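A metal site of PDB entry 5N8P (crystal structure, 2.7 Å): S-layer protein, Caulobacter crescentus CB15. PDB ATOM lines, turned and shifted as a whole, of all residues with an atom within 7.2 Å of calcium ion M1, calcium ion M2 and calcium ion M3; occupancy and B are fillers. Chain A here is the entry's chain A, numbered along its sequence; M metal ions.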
ATOM      1  N   VAL A 613     -22.821  13.731   5.946  1.00  0.00           N
ATOM      2  CA  VAL A 613     -21.899  13.184   4.964  1.00  0.00           C
ATOM      3  C   VAL A 613     -20.628  14.002   4.871  1.00  0.00           C
ATOM      4  O   VAL A 613     -20.623  15.209   4.774  1.00  0.00           O
ATOM      5  CB  VAL A 613     -22.530  13.061   3.581  1.00  0.00           C
ATOM      6  CG1 VAL A 613     -21.682  12.149   2.728  1.00  0.00           C
ATOM      7  CG2 VAL A 613     -23.933  12.511   3.731  1.00  0.00           C
ATOM      8  N   ASN A 615     -18.108  12.163   3.161  1.00  0.00           N
ATOM      9  CA  ASN A 615     -17.541  11.296   2.132  1.00  0.00           C
ATOM     10  C   ASN A 615     -17.235  12.005   0.813  1.00  0.00           C
ATOM     11  O   ASN A 615     -18.051  12.741   0.326  1.00  0.00           O
ATOM     12  CB  ASN A 615     -18.519  10.132   1.898  1.00  0.00           C
ATOM     13  CG  ASN A 615     -17.980   9.095   0.918  1.00  0.00           C
ATOM     14  OD1 ASN A 615     -17.751   9.389  -0.248  1.00  0.00           O
ATOM     15  ND2 ASN A 615     -17.814   7.866   1.395  1.00  0.00           N
ATOM     16  N   VAL A 617     -16.772  10.855  -2.465  1.00  0.00           N
ATOM     17  CA  VAL A 617     -17.566  10.518  -3.644  1.00  0.00           C
ATOM     18  C   VAL A 617     -19.001  10.935  -3.387  1.00  0.00           C
ATOM     19  O   VAL A 617     -19.677  11.413  -4.272  1.00  0.00           O
ATOM     20  CB  VAL A 617     -17.381   9.036  -4.040  1.00  0.00           C
ATOM     21  CG1 VAL A 617     -18.397   8.567  -5.090  1.00  0.00           C
ATOM     22  CG2 VAL A 617     -15.953   8.821  -4.528  1.00  0.00           C
ATOM     23  N   GLY A 618     -19.435  10.773  -2.145  1.00  0.00           N
ATOM     24  CA  GLY A 618     -20.785  11.146  -1.754  1.00  0.00           C
ATOM     25  C   GLY A 618     -21.576  10.018  -1.161  1.00  0.00           C
ATOM     26  O   GLY A 618     -21.086   8.897  -1.029  1.00  0.00           O
ATOM     27  N   PHE A 631     -29.892  17.507   7.489  1.00  0.00           N
ATOM     28  CA  PHE A 631     -28.937  16.806   6.659  1.00  0.00           C
ATOM     29  C   PHE A 631     -27.826  17.742   6.235  1.00  0.00           C
ATOM     30  O   PHE A 631     -28.083  18.827   5.829  1.00  0.00           O
ATOM     31  CB  PHE A 631     -29.631  16.224   5.411  1.00  0.00           C
ATOM     32  CG  PHE A 631     -28.675  15.556   4.443  1.00  0.00           C
ATOM     33  CD1 PHE A 631     -28.475  14.184   4.482  1.00  0.00           C
ATOM     34  CD2 PHE A 631     -27.948  16.309   3.511  1.00  0.00           C
ATOM     35  CE1 PHE A 631     -27.588  13.563   3.631  1.00  0.00           C
ATOM     36  CE2 PHE A 631     -27.053  15.700   2.643  1.00  0.00           C
ATOM     37  CZ  PHE A 631     -26.880  14.328   2.704  1.00  0.00           C
ATOM     38  N   THR A 632     -26.599  17.276   6.282  1.00  0.00           N
ATOM     39  CA  THR A 632     -25.463  18.085   5.817  1.00  0.00           C
ATOM     40  C   THR A 632     -24.584  17.272   4.855  1.00  0.00           C
ATOM     41  O   THR A 632     -24.060  16.253   5.234  1.00  0.00           O
ATOM     42  CB  THR A 632     -24.678  18.607   7.041  1.00  0.00           C
ATOM     43  OG1 THR A 632     -25.606  19.051   8.024  1.00  0.00           O
ATOM     44  CG2 THR A 632     -23.719  19.720   6.658  1.00  0.00           C
ATOM     45  N   GLY A 633     -24.474  17.704   3.605  1.00  0.00           N
ATOM     46  CA  GLY A 633     -23.559  17.076   2.632  1.00  0.00           C
ATOM     47  C   GLY A 633     -22.118  17.550   2.808  1.00  0.00           C
ATOM     48  O   GLY A 633     -21.842  18.446   3.634  1.00  0.00           O
ATOM     49  N   GLY A 634     -21.197  16.960   2.046  1.00  0.00           N
ATOM     50  CA  GLY A 634     -19.775  17.383   1.995  1.00  0.00           C
ATOM     51  C   GLY A 634     -19.429  17.623   0.558  1.00  0.00           C
ATOM     52  O   GLY A 634     -20.345  17.923  -0.227  1.00  0.00           O
ATOM     53  N   ALA A 635     -18.152  17.517   0.159  1.00  0.00           N
ATOM     54  CA  ALA A 635     -17.787  17.460  -1.271  1.00  0.00           C
ATOM     55  C   ALA A 635     -18.478  16.239  -1.885  1.00  0.00           C
ATOM     56  O   ALA A 635     -19.031  15.430  -1.171  1.00  0.00           O
ATOM     57  CB  ALA A 635     -16.268  17.423  -1.468  1.00  0.00           C
ATOM     58  N   GLY A 636     -18.498  16.135  -3.205  1.00  0.00           N
ATOM     59  CA  GLY A 636     -19.059  14.932  -3.833  1.00  0.00           C
ATOM     60  C   GLY A 636     -20.567  14.752  -3.834  1.00  0.00           C
ATOM     61  O   GLY A 636     -21.289  15.231  -2.944  1.00  0.00           O
ATOM     62  N   ALA A 637     -21.032  14.018  -4.841  1.00  0.00           N
ATOM     63  CA  ALA A 637     -22.435  13.948  -5.229  1.00  0.00           C
ATOM     64  C   ALA A 637     -23.269  13.323  -4.136  1.00  0.00           C
ATOM     65  O   ALA A 637     -23.439  12.118  -4.125  1.00  0.00           O
ATOM     66  CB  ALA A 637     -22.610  13.199  -6.567  1.00  0.00           C
ATOM     67  N   ASP A 638     -23.749  14.115  -3.192  1.00  0.00           N
ATOM     68  CA  ASP A 638     -24.655  13.564  -2.198  1.00  0.00           C
ATOM     69  C   ASP A 638     -26.077  13.589  -2.784  1.00  0.00           C
ATOM     70  O   ASP A 638     -26.321  14.341  -3.729  1.00  0.00           O
ATOM     71  CB  ASP A 638     -24.516  14.284  -0.839  1.00  0.00           C
ATOM     72  CG  ASP A 638     -23.041  14.545  -0.427  1.00  0.00           C
ATOM     73  OD1 ASP A 638     -22.279  13.601  -0.167  1.00  0.00           O
ATOM     74  OD2 ASP A 638     -22.634  15.724  -0.372  1.00  0.00           O
ATOM     75  N   SER A 639     -27.002  12.754  -2.287  1.00  0.00           N
ATOM     76  CA  SER A 639     -28.339  12.628  -2.925  1.00  0.00           C
ATOM     77  C   SER A 639     -29.486  12.071  -2.074  1.00  0.00           C
ATOM     78  O   SER A 639     -29.490  10.893  -1.718  1.00  0.00           O
ATOM     79  CB  SER A 639     -28.255  11.870  -4.234  1.00  0.00           C
ATOM     80  OG  SER A 639     -29.524  11.370  -4.583  1.00  0.00           O
ATOM     81  N   VAL A 650     -28.318  21.564   4.007  1.00  0.00           N
ATOM     82  CA  VAL A 650     -27.175  22.029   3.226  1.00  0.00           C
ATOM     83  C   VAL A 650     -26.604  20.852   2.480  1.00  0.00           C
ATOM     84  O   VAL A 650     -26.643  19.754   2.979  1.00  0.00           O
ATOM     85  CB  VAL A 650     -26.054  22.723   4.056  1.00  0.00           C
ATOM     86  CG1 VAL A 650     -25.068  23.458   3.116  1.00  0.00           C
ATOM     87  CG2 VAL A 650     -26.664  23.710   5.058  1.00  0.00           C
ATOM     88  N   MET A 651     -26.069  21.091   1.281  1.00  0.00           N
ATOM     89  CA  MET A 651     -25.669  20.042   0.404  1.00  0.00           C
ATOM     90  C   MET A 651     -24.190  20.018   0.147  1.00  0.00           C
ATOM     91  O   MET A 651     -23.692  19.029  -0.413  1.00  0.00           O
ATOM     92  CB  MET A 651     -26.405  20.168  -0.897  1.00  0.00           C
ATOM     93  CG  MET A 651     -27.143  18.931  -1.302  1.00  0.00           C
ATOM     94  SD  MET A 651     -28.303  18.418  -0.043  1.00  0.00           S
ATOM     95  CE  MET A 651     -28.653  16.751  -0.647  1.00  0.00           C
ATOM     96  N   GLY A 652     -23.480  21.083   0.545  1.00  0.00           N
ATOM     97  CA  GLY A 652     -22.003  21.164   0.386  1.00  0.00           C
ATOM     98  C   GLY A 652     -21.557  21.296  -1.063  1.00  0.00           C
ATOM     99  O   GLY A 652     -22.373  21.592  -1.937  1.00  0.00           O
ATOM    100  N   ALA A 653     -20.270  21.064  -1.320  1.00  0.00           N
ATOM    101  CA  ALA A 653     -19.706  21.107  -2.687  1.00  0.00           C
ATOM    102  C   ALA A 653     -20.113  19.889  -3.537  1.00  0.00           C
ATOM    103  O   ALA A 653     -20.882  19.052  -3.084  1.00  0.00           O
ATOM    104  CB  ALA A 653     -18.176  21.277  -2.658  1.00  0.00           C
ATOM    105  N   GLY A 654     -19.624  19.828  -4.785  1.00  0.00           N
ATOM    106  CA  GLY A 654     -19.889  18.717  -5.699  1.00  0.00           C
ATOM    107  C   GLY A 654     -21.299  18.613  -6.252  1.00  0.00           C
ATOM    108  O   GLY A 654     -22.214  19.296  -5.798  1.00  0.00           O
ATOM    109  N   ASP A 655     -21.511  17.735  -7.211  1.00  0.00           N
ATOM    110  CA  ASP A 655     -22.751  17.732  -7.950  1.00  0.00           C
ATOM    111  C   ASP A 655     -23.904  16.948  -7.301  1.00  0.00           C
ATOM    112  O   ASP A 655     -24.138  15.763  -7.575  1.00  0.00           O
ATOM    113  CB  ASP A 655     -22.450  17.350  -9.395  1.00  0.00           C
ATOM    114  CG  ASP A 655     -21.517  18.360 -10.069  1.00  0.00           C
ATOM    115  OD1 ASP A 655     -21.335  18.202 -11.303  1.00  0.00           O
ATOM    116  OD2 ASP A 655     -20.973  19.306  -9.406  1.00  0.00           O
ATOM    117  N   ASP A 656     -24.631  17.659  -6.445  1.00  0.00           N
ATOM    118  CA  ASP A 656     -25.615  17.050  -5.540  1.00  0.00           C
ATOM    119  C   ASP A 656     -26.997  16.916  -6.160  1.00  0.00           C
ATOM    120  O   ASP A 656     -27.240  17.481  -7.214  1.00  0.00           O
ATOM    121  CB  ASP A 656     -25.688  17.898  -4.281  1.00  0.00           C
ATOM    122  CG  ASP A 656     -24.394  17.884  -3.484  1.00  0.00           C
ATOM    123  OD1 ASP A 656     -24.032  16.821  -2.928  1.00  0.00           O
ATOM    124  OD2 ASP A 656     -23.726  18.944  -3.370  1.00  0.00           O
ATOM    125  N   THR A 657     -27.905  16.188  -5.510  1.00  0.00           N
ATOM    126  CA  THR A 657     -29.271  15.949  -6.065  1.00  0.00           C
ATOM    127  C   THR A 657     -30.354  15.830  -4.969  1.00  0.00           C
ATOM    128  O   THR A 657     -30.440  14.785  -4.308  1.00  0.00           O
ATOM    129  CB  THR A 657     -29.323  14.650  -6.906  1.00  0.00           C
ATOM    130  OG1 THR A 657     -28.239  14.644  -7.816  1.00  0.00           O
ATOM    131  CG2 THR A 657     -30.624  14.605  -7.748  1.00  0.00           C
ATOM    132  N   ASN A 672     -30.211  24.422   0.533  1.00  0.00           N
ATOM    133  CA  ASN A 672     -29.223  25.045  -0.312  1.00  0.00           C
ATOM    134  C   ASN A 672     -28.338  23.979  -0.979  1.00  0.00           C
ATOM    135  O   ASN A 672     -27.688  23.204  -0.303  1.00  0.00           O
ATOM    136  CB  ASN A 672     -28.414  26.115   0.478  1.00  0.00           C
ATOM    137  CG  ASN A 672     -27.156  26.611  -0.279  1.00  0.00           C
ATOM    138  OD1 ASN A 672     -27.182  26.904  -1.467  1.00  0.00           O
ATOM    139  ND2 ASN A 672     -26.053  26.738   0.446  1.00  0.00           N
ATOM    140  N   GLY A 673     -28.350  23.933  -2.308  1.00  0.00           N
ATOM    141  CA  GLY A 673     -27.464  23.101  -3.094  1.00  0.00           C
ATOM    142  C   GLY A 673     -25.962  23.298  -2.935  1.00  0.00           C
ATOM    143  O   GLY A 673     -25.209  22.432  -3.379  1.00  0.00           O
ATOM    144  N   GLY A 674     -25.502  24.405  -2.304  1.00  0.00           N
ATOM    145  CA  GLY A 674     -24.056  24.719  -2.151  1.00  0.00           C
ATOM    146  C   GLY A 674     -23.303  24.873  -3.493  1.00  0.00           C
ATOM    147  O   GLY A 674     -23.909  25.042  -4.538  1.00  0.00           O
ATOM    148  N   ASP A 675     -21.983  24.821  -3.458  1.00  0.00           N
ATOM    149  CA  ASP A 675     -21.162  24.903  -4.679  1.00  0.00           C
ATOM    150  C   ASP A 675     -21.363  23.735  -5.660  1.00  0.00           C
ATOM    151  O   ASP A 675     -21.803  22.642  -5.258  1.00  0.00           O
ATOM    152  CB  ASP A 675     -19.669  24.974  -4.345  1.00  0.00           C
ATOM    153  CG  ASP A 675     -19.284  26.190  -3.549  1.00  0.00           C
ATOM    154  OD1 ASP A 675     -20.213  26.926  -3.094  1.00  0.00           O
ATOM    155  OD2 ASP A 675     -18.050  26.377  -3.384  1.00  0.00           O
ATOM    156  N   GLY A 676     -21.019  23.980  -6.933  1.00  0.00           N
ATOM    157  CA  GLY A 676     -21.092  22.955  -7.995  1.00  0.00           C
ATOM    158  C   GLY A 676     -22.430  22.909  -8.708  1.00  0.00           C
ATOM    159  O   GLY A 676     -23.354  23.658  -8.367  1.00  0.00           O
ATOM    160  N   THR A 677     -22.548  22.037  -9.697  1.00  0.00           N
ATOM    161  CA  THR A 677     -23.773  21.975 -10.481  1.00  0.00           C
ATOM    162  C   THR A 677     -24.697  20.997  -9.815  1.00  0.00           C
ATOM    163  O   THR A 677     -24.451  19.789  -9.839  1.00  0.00           O
ATOM    164  CB  THR A 677     -23.476  21.556 -11.931  1.00  0.00           C
ATOM    165  OG1 THR A 677     -22.370  22.336 -12.397  1.00  0.00           O
ATOM    166  CG2 THR A 677     -24.666  21.819 -12.830  1.00  0.00           C
ATOM    167  N   ASP A 678     -25.780  21.505  -9.228  1.00  0.00           N
ATOM    168  CA  ASP A 678     -26.664  20.662  -8.420  1.00  0.00           C
ATOM    169  C   ASP A 678     -28.024  20.553  -9.040  1.00  0.00           C
ATOM    170  O   ASP A 678     -28.565  21.546  -9.496  1.00  0.00           O
ATOM    171  CB  ASP A 678     -26.790  21.231  -7.005  1.00  0.00           C
ATOM    172  CG  ASP A 678     -25.454  21.601  -6.396  1.00  0.00           C
ATOM    173  OD1 ASP A 678     -24.731  20.678  -5.944  1.00  0.00           O
ATOM    174  OD2 ASP A 678     -25.137  22.827  -6.343  1.00  0.00           O
ATOM    175  N   GLY A 696     -31.963  27.529  -2.903  1.00  0.00           N
ATOM    176  CA  GLY A 696     -30.860  28.317  -3.484  1.00  0.00           C
ATOM    177  C   GLY A 696     -29.700  27.416  -3.899  1.00  0.00           C
ATOM    178  O   GLY A 696     -29.612  26.271  -3.409  1.00  0.00           O
ATOM    179  N   GLY A 697     -28.811  27.888  -4.785  1.00  0.00           N
ATOM    180  CA  GLY A 697     -27.617  27.091  -5.167  1.00  0.00           C
ATOM    181  C   GLY A 697     -27.827  25.935  -6.132  1.00  0.00           C
ATOM    182  O   GLY A 697     -26.916  25.131  -6.388  1.00  0.00           O
ATOM    183  N   PHE A 698     -29.040  25.847  -6.689  1.00  0.00           N
ATOM    184  CA  PHE A 698     -29.378  24.870  -7.732  1.00  0.00           C
ATOM    185  C   PHE A 698     -29.174  25.415  -9.152  1.00  0.00           C
ATOM    186  O   PHE A 698     -29.284  26.607  -9.373  1.00  0.00           O
ATOM    187  CB  PHE A 698     -30.809  24.351  -7.516  1.00  0.00           C
ATOM    188  CG  PHE A 698     -30.923  23.463  -6.325  1.00  0.00           C
ATOM    189  CD1 PHE A 698     -30.578  22.107  -6.420  1.00  0.00           C
ATOM    190  CD2 PHE A 698     -31.292  23.980  -5.094  1.00  0.00           C
ATOM    191  CE1 PHE A 698     -30.630  21.284  -5.299  1.00  0.00           C
ATOM    192  CE2 PHE A 698     -31.357  23.165  -3.982  1.00  0.00           C
ATOM    193  CZ  PHE A 698     -31.012  21.813  -4.086  1.00  0.00           C
ATOM    194  N   GLU A 699     -28.854  24.525 -10.082  1.00  0.00           N
ATOM    195  CA  GLU A 699     -28.482  24.932 -11.439  1.00  0.00           C
ATOM    196  C   GLU A 699     -29.314  24.218 -12.471  1.00  0.00           C
ATOM    197  O   GLU A 699     -29.453  24.727 -13.570  1.00  0.00           O
ATOM    198  CB  GLU A 699     -27.006  24.659 -11.691  1.00  0.00           C
ATOM    199  CG  GLU A 699     -26.060  25.642 -11.034  1.00  0.00           C
ATOM    200  CD  GLU A 699     -25.837  25.400  -9.543  1.00  0.00           C
ATOM    201  OE1 GLU A 699     -26.145  24.314  -8.976  1.00  0.00           O
ATOM    202  OE2 GLU A 699     -25.310  26.341  -8.894  1.00  0.00           O
HETATM  203 CA    CA M   1     -24.582  25.280  -6.973  1.00  0.00          CA
HETATM  204 CA    CA M   2     -23.303  21.045  -4.221  1.00  0.00          CA
HETATM  205 CA    CA M   3     -22.083  17.479  -1.571  1.00  0.00          CA
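O of Ala 635 touches calcium ion M3, at 3.7 Å. Eight residues have an atom within 4 Å of calcium ion M3: Gly 634, Ala 635, Gly 636, Asp 638, Met 651, Gly 652, Ala 653 and Asp 656.
Calcium ion M2 is bound by the side-chain carboxylate (OD1) of Asp 678 (2.3 Å), the side-chain carboxylate (OD2) of Asp 656 (2.3 Å), the backbone carbonyl oxygen (O) of Asp 675 (2.4 Å), the backbone carbonyl oxygen (O) of Gly 673 (2.5 Å), the backbone carbonyl oxygen (O) of Gly 652 (2.5 Å) and the backbone carbonyl oxygen (O) of Gly 654 (2.6 Å).
Calcium ion M1 is bound by OE2 of Glu 699 (2.3 Å), O of Gly 697 (2.4 Å), O of Gly 676 (2.5 Å), O of Gly 674 (2.5 Å), OD2 of Asp 678 (2.6 Å) and OE1 of Glu 699 (2.7 Å). Calcium ion M1 has six donor atoms within binding distance.
Calcium ion M3 is bound by OD2 of Asp 638, O of Gly 634, OD1 of Asp 656, O of Ala 653, O of Met 651, O of Gly 636 and OD2 of Asp 656. Calcium ion M3 has seven donor atoms within binding distance.
Six residues have an atom within 4 Å of calcium ion M1: Gly 674, Asp 675, Gly 676, Asp 678, Gly 697 and Glu 699.
Of the 32 residues printed, 8 come within 4 Å of calcium ion M2. The nearest printed residue that does not touch calcium ion M2 is Met 651 (4.3 Å).
N of Thr 657 sits at hydrogen-bond distance from O of Asp 638, 3.0 Å away. The backbone NH of Gly 634 lies within hydrogen-bond range of the backbone carbonyl oxygen of Val 613, 3.3 Å away. N of Gly 673 lies within hydrogen-bond range of O of Gly 696, at 2.9 Å. N of Met 651 sits at hydrogen-bond distance from O of Asn 672 (3.1 Å). OD1 of Asn 672 lies within hydrogen-bond range of N of Gly 674.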
